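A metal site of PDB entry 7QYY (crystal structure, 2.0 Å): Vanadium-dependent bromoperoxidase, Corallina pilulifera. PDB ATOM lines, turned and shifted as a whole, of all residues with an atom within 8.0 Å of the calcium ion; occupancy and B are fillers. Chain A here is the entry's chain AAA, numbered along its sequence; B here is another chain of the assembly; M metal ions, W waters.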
ATOM      1  N   PRO A 360     -21.235   3.829 -19.981  1.00  0.00           N
ATOM      2  CA  PRO A 360     -21.857   5.033 -19.429  1.00  0.00           C
ATOM      3  C   PRO A 360     -21.208   5.324 -18.079  1.00  0.00           C
ATOM      4  O   PRO A 360     -20.604   4.430 -17.477  1.00  0.00           O
ATOM      5  CB  PRO A 360     -23.337   4.651 -19.155  1.00  0.00           C
ATOM      6  CG  PRO A 360     -23.437   3.145 -19.434  1.00  0.00           C
ATOM      7  CD  PRO A 360     -22.025   2.611 -19.699  1.00  0.00           C
ATOM      8  N   PHE A 361     -21.370   6.577 -17.619  1.00  0.00           N
ATOM      9  CA  PHE A 361     -21.076   6.990 -16.243  1.00  0.00           C
ATOM     10  C   PHE A 361     -19.569   7.024 -15.951  1.00  0.00           C
ATOM     11  O   PHE A 361     -19.154   7.095 -14.782  1.00  0.00           O
ATOM     12  CB  PHE A 361     -21.860   6.167 -15.218  1.00  0.00           C
ATOM     13  CG  PHE A 361     -23.346   6.087 -15.510  1.00  0.00           C
ATOM     14  CD1 PHE A 361     -24.075   7.245 -15.814  1.00  0.00           C
ATOM     15  CD2 PHE A 361     -24.029   4.862 -15.430  1.00  0.00           C
ATOM     16  CE1 PHE A 361     -25.447   7.186 -16.059  1.00  0.00           C
ATOM     17  CE2 PHE A 361     -25.410   4.799 -15.655  1.00  0.00           C
ATOM     18  CZ  PHE A 361     -26.117   5.957 -15.980  1.00  0.00           C
ATOM     19  N   GLN A 362     -18.740   6.974 -16.991  1.00  0.00           N
ATOM     20  CA  GLN A 362     -17.309   6.906 -16.755  1.00  0.00           C
ATOM     21  C   GLN A 362     -16.686   8.303 -16.546  1.00  0.00           C
ATOM     22  O   GLN A 362     -15.488   8.402 -16.348  1.00  0.00           O
ATOM     23  CB  GLN A 362     -16.568   6.118 -17.838  1.00  0.00           C
ATOM     24  CG  GLN A 362     -17.142   4.732 -18.078  1.00  0.00           C
ATOM     25  CD  GLN A 362     -17.110   3.829 -16.871  1.00  0.00           C
ATOM     26  OE1 GLN A 362     -16.168   3.857 -16.055  1.00  0.00           O
ATOM     27  NE2 GLN A 362     -18.154   2.998 -16.780  1.00  0.00           N
ATOM     28  N   GLN A 363     -17.485   9.398 -16.557  1.00  0.00           N
ATOM     29  CA  GLN A 363     -16.936  10.716 -16.356  1.00  0.00           C
ATOM     30  C   GLN A 363     -16.794  10.970 -14.853  1.00  0.00           C
ATOM     31  O   GLN A 363     -17.340  10.213 -14.035  1.00  0.00           O
ATOM     32  CB  GLN A 363     -17.853  11.784 -16.944  1.00  0.00           C
ATOM     33  CG  GLN A 363     -17.789  11.704 -18.464  1.00  0.00           C
ATOM     34  CD  GLN A 363     -18.838  12.555 -19.085  1.00  0.00           C
ATOM     35  OE1 GLN A 363     -20.002  12.152 -19.259  1.00  0.00           O
ATOM     36  NE2 GLN A 363     -18.423  13.775 -19.338  1.00  0.00           N
ATOM     37  N   GLU A 364     -16.104  12.069 -14.511  1.00  0.00           N
ATOM     38  CA  GLU A 364     -16.095  12.547 -13.150  1.00  0.00           C
ATOM     39  C   GLU A 364     -17.524  12.754 -12.688  1.00  0.00           C
ATOM     40  O   GLU A 364     -18.325  13.279 -13.439  1.00  0.00           O
ATOM     41  CB  GLU A 364     -15.355  13.877 -13.033  1.00  0.00           C
ATOM     42  CG  GLU A 364     -13.871  13.643 -13.235  1.00  0.00           C
ATOM     43  CD  GLU A 364     -13.068  14.883 -12.838  1.00  0.00           C
ATOM     44  OE1 GLU A 364     -11.815  14.774 -12.897  1.00  0.00           O
ATOM     45  OE2 GLU A 364     -13.680  15.958 -12.463  1.00  0.00           O
ATOM     46  N   ASP A 365     -17.817  12.361 -11.453  1.00  0.00           N
ATOM     47  CA  ASP A 365     -19.179  12.356 -10.959  1.00  0.00           C
ATOM     48  C   ASP A 365     -19.758  13.764 -10.861  1.00  0.00           C
ATOM     49  O   ASP A 365     -20.995  13.902 -10.914  1.00  0.00           O
ATOM     50  CB  ASP A 365     -19.275  11.592  -9.642  1.00  0.00           C
ATOM     51  CG  ASP A 365     -18.992  10.122  -9.861  1.00  0.00           C
ATOM     52  OD1 ASP A 365     -18.925   9.658 -11.054  1.00  0.00           O
ATOM     53  OD2 ASP A 365     -18.905   9.441  -8.870  1.00  0.00           O
ATOM     54  N   LYS A 366     -18.892  14.800 -10.772  1.00  0.00           N
ATOM     55  CA  LYS A 366     -19.438  16.156 -10.784  1.00  0.00           C
ATOM     56  C   LYS A 366     -20.121  16.434 -12.124  1.00  0.00           C
ATOM     57  O   LYS A 366     -21.046  17.248 -12.196  1.00  0.00           O
ATOM     58  CB  LYS A 366     -18.344  17.211 -10.541  1.00  0.00           C
ATOM     59  CG  LYS A 366     -17.311  17.355 -11.640  1.00  0.00           C
ATOM     60  CD  LYS A 366     -16.245  18.453 -11.307  1.00  0.00           C
ATOM     61  CE  LYS A 366     -15.136  18.512 -12.346  1.00  0.00           C
ATOM     62  NZ  LYS A 366     -13.775  18.734 -11.783  1.00  0.00           N
ATOM     63  N   LEU A 367     -19.696  15.686 -13.170  1.00  0.00           N
ATOM     64  CA  LEU A 367     -20.346  15.825 -14.478  1.00  0.00           C
ATOM     65  C   LEU A 367     -21.543  14.899 -14.661  1.00  0.00           C
ATOM     66  O   LEU A 367     -22.621  15.351 -15.143  1.00  0.00           O
ATOM     67  CB  LEU A 367     -19.327  15.598 -15.579  1.00  0.00           C
ATOM     68  CG  LEU A 367     -18.156  16.566 -15.566  1.00  0.00           C
ATOM     69  CD1 LEU A 367     -17.226  16.264 -16.754  1.00  0.00           C
ATOM     70  CD2 LEU A 367     -18.656  18.010 -15.611  1.00  0.00           C
ATOM     71  N   ASP A 368     -21.393  13.613 -14.320  1.00  0.00           N
ATOM     72  CA  ASP A 368     -22.455  12.672 -14.656  1.00  0.00           C
ATOM     73  C   ASP A 368     -23.367  12.298 -13.466  1.00  0.00           C
ATOM     74  O   ASP A 368     -24.366  11.586 -13.648  1.00  0.00           O
ATOM     75  CB  ASP A 368     -21.884  11.443 -15.407  1.00  0.00           C
ATOM     76  CG  ASP A 368     -20.851  10.641 -14.607  1.00  0.00           C
ATOM     77  OD1 ASP A 368     -20.742  10.757 -13.341  1.00  0.00           O
ATOM     78  OD2 ASP A 368     -20.173   9.783 -15.228  1.00  0.00           O
ATOM     79  N   ASN A 369     -23.000  12.689 -12.222  1.00  0.00           N
ATOM     80  CA  ASN A 369     -23.732  12.333 -10.997  1.00  0.00           C
ATOM     81  C   ASN A 369     -23.854  10.808 -10.885  1.00  0.00           C
ATOM     82  O   ASN A 369     -24.823  10.326 -10.281  1.00  0.00           O
ATOM     83  CB  ASN A 369     -25.165  12.921 -10.952  1.00  0.00           C
ATOM     84  CG  ASN A 369     -25.177  14.441 -10.841  1.00  0.00           C
ATOM     85  OD1 ASN A 369     -24.190  15.005 -10.426  1.00  0.00           O
ATOM     86  ND2 ASN A 369     -26.217  15.120 -11.298  1.00  0.00           N
ATOM     87  N   GLN A 370     -22.912  10.030 -11.453  1.00  0.00           N
ATOM     88  CA  GLN A 370     -23.168   8.597 -11.390  1.00  0.00           C
ATOM     89  C   GLN A 370     -21.859   7.808 -11.387  1.00  0.00           C
ATOM     90  O   GLN A 370     -21.035   7.966 -12.271  1.00  0.00           O
ATOM     91  CB  GLN A 370     -24.049   8.154 -12.560  1.00  0.00           C
ATOM     92  CG  GLN A 370     -24.539   6.711 -12.411  1.00  0.00           C
ATOM     93  CD  GLN A 370     -25.767   6.518 -11.537  1.00  0.00           C
ATOM     94  OE1 GLN A 370     -26.283   5.405 -11.473  1.00  0.00           O
ATOM     95  NE2 GLN A 370     -26.311   7.560 -10.893  1.00  0.00           N
ATOM     96  N   ASP A 371     -21.682   6.960 -10.365  1.00  0.00           N
ATOM     97  CA  ASP A 371     -20.526   6.077 -10.287  1.00  0.00           C
ATOM     98  C   ASP A 371     -21.028   4.669 -10.628  1.00  0.00           C
ATOM     99  O   ASP A 371     -22.245   4.429 -10.753  1.00  0.00           O
ATOM    100  CB  ASP A 371     -19.984   6.154  -8.851  1.00  0.00           C
ATOM    101  CG  ASP A 371     -18.597   5.590  -8.604  1.00  0.00           C
ATOM    102  OD1 ASP A 371     -17.985   5.042  -9.549  1.00  0.00           O
ATOM    103  OD2 ASP A 371     -18.131   5.696  -7.427  1.00  0.00           O
ATOM    104  N   VAL A 372     -20.094   3.725 -10.783  1.00  0.00           N
ATOM    105  CA  VAL A 372     -20.420   2.441 -11.401  1.00  0.00           C
ATOM    106  C   VAL A 372     -19.963   1.293 -10.500  1.00  0.00           C
ATOM    107  O   VAL A 372     -18.915   1.391  -9.837  1.00  0.00           O
ATOM    108  CB  VAL A 372     -19.817   2.327 -12.814  1.00  0.00           C
ATOM    109  CG1 VAL A 372     -20.531   3.288 -13.786  1.00  0.00           C
ATOM    110  CG2 VAL A 372     -18.296   2.498 -12.835  1.00  0.00           C
ATOM    111  N   ARG B 123     -18.826  12.665  -4.981  1.00  0.00           N
ATOM    112  CA  ARG B 123     -18.955  11.341  -5.573  1.00  0.00           C
ATOM    113  C   ARG B 123     -20.431  11.167  -5.913  1.00  0.00           C
ATOM    114  O   ARG B 123     -21.276  11.792  -5.264  1.00  0.00           O
ATOM    115  CB  ARG B 123     -18.476  10.270  -4.584  1.00  0.00           C
ATOM    116  CG  ARG B 123     -19.225  10.338  -3.256  1.00  0.00           C
ATOM    117  CD  ARG B 123     -18.750   9.176  -2.345  1.00  0.00           C
ATOM    118  NE  ARG B 123     -18.956   7.871  -2.966  1.00  0.00           N
ATOM    119  CZ  ARG B 123     -18.896   6.678  -2.354  1.00  0.00           C
ATOM    120  NH1 ARG B 123     -18.736   6.641  -1.037  1.00  0.00           N
ATOM    121  NH2 ARG B 123     -19.028   5.540  -3.060  1.00  0.00           N
ATOM    122  N   GLY B 124     -20.750  10.315  -6.900  1.00  0.00           N
ATOM    123  CA  GLY B 124     -22.142  10.189  -7.343  1.00  0.00           C
ATOM    124  C   GLY B 124     -22.773   8.848  -6.972  1.00  0.00           C
ATOM    125  O   GLY B 124     -22.083   7.927  -6.502  1.00  0.00           O
ATOM    126  N   TRP B 125     -24.092   8.748  -7.198  1.00  0.00           N
ATOM    127  CA  TRP B 125     -24.828   7.533  -6.907  1.00  0.00           C
ATOM    128  C   TRP B 125     -24.297   6.362  -7.738  1.00  0.00           C
ATOM    129  O   TRP B 125     -23.913   6.544  -8.912  1.00  0.00           O
ATOM    130  CB  TRP B 125     -26.321   7.782  -7.115  1.00  0.00           C
ATOM    131  CG  TRP B 125     -26.754   8.867  -6.174  1.00  0.00           C
ATOM    132  CD1 TRP B 125     -26.944   8.733  -4.827  1.00  0.00           C
ATOM    133  CD2 TRP B 125     -27.038  10.255  -6.494  1.00  0.00           C
ATOM    134  NE1 TRP B 125     -27.383   9.922  -4.298  1.00  0.00           N
ATOM    135  CE2 TRP B 125     -27.413  10.884  -5.276  1.00  0.00           C
ATOM    136  CE3 TRP B 125     -27.025  11.015  -7.679  1.00  0.00           C
ATOM    137  CZ2 TRP B 125     -27.711  12.258  -5.205  1.00  0.00           C
ATOM    138  CZ3 TRP B 125     -27.292  12.370  -7.598  1.00  0.00           C
ATOM    139  CH2 TRP B 125     -27.631  12.993  -6.381  1.00  0.00           C
HETATM  140 CA    CA M   1     -19.136   8.892 -13.226  1.00  0.00          CA
HETATM  141  O   HOH W   1     -17.561   7.305 -12.444  1.00  0.00           O
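O of Trp 125 of chain B lies close to NE2 of Gln 370 (3.3 Å). The backbone NH of Gly 124 of chain B sits at hydrogen-bond distance from the side-chain carboxylate of Asp 365, 2.8 Å away. The side-chain amide oxygen (OD1) of Asn 369 sits close to the backbone carbonyl oxygen (O) of Asp 365, at 3.4 Å.
OD1 of Asp 365 binds the calcium ion (2.3 Å). The calcium ion is bound by the backbone carbonyl oxygen (O) of Gln 370, at 2.3 Å. Water W1 binds the calcium ion, 2.4 Å away. The calcium ion is bound by O of Gln 363. The calcium ion is bound by the backbone carbonyl oxygen (O) of Phe 361, at 2.4 Å. OD2 of Asp 368 is bound to the calcium ion (2.4 Å). The calcium ion is bound by OD1 of Asp 368 (2.5 Å). The calcium ion has seven donor atoms within binding distance.
Within 4 Å of the calcium ion: Phe 361, Gln 363, Asp 365, Asp 368 and Gln 370.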
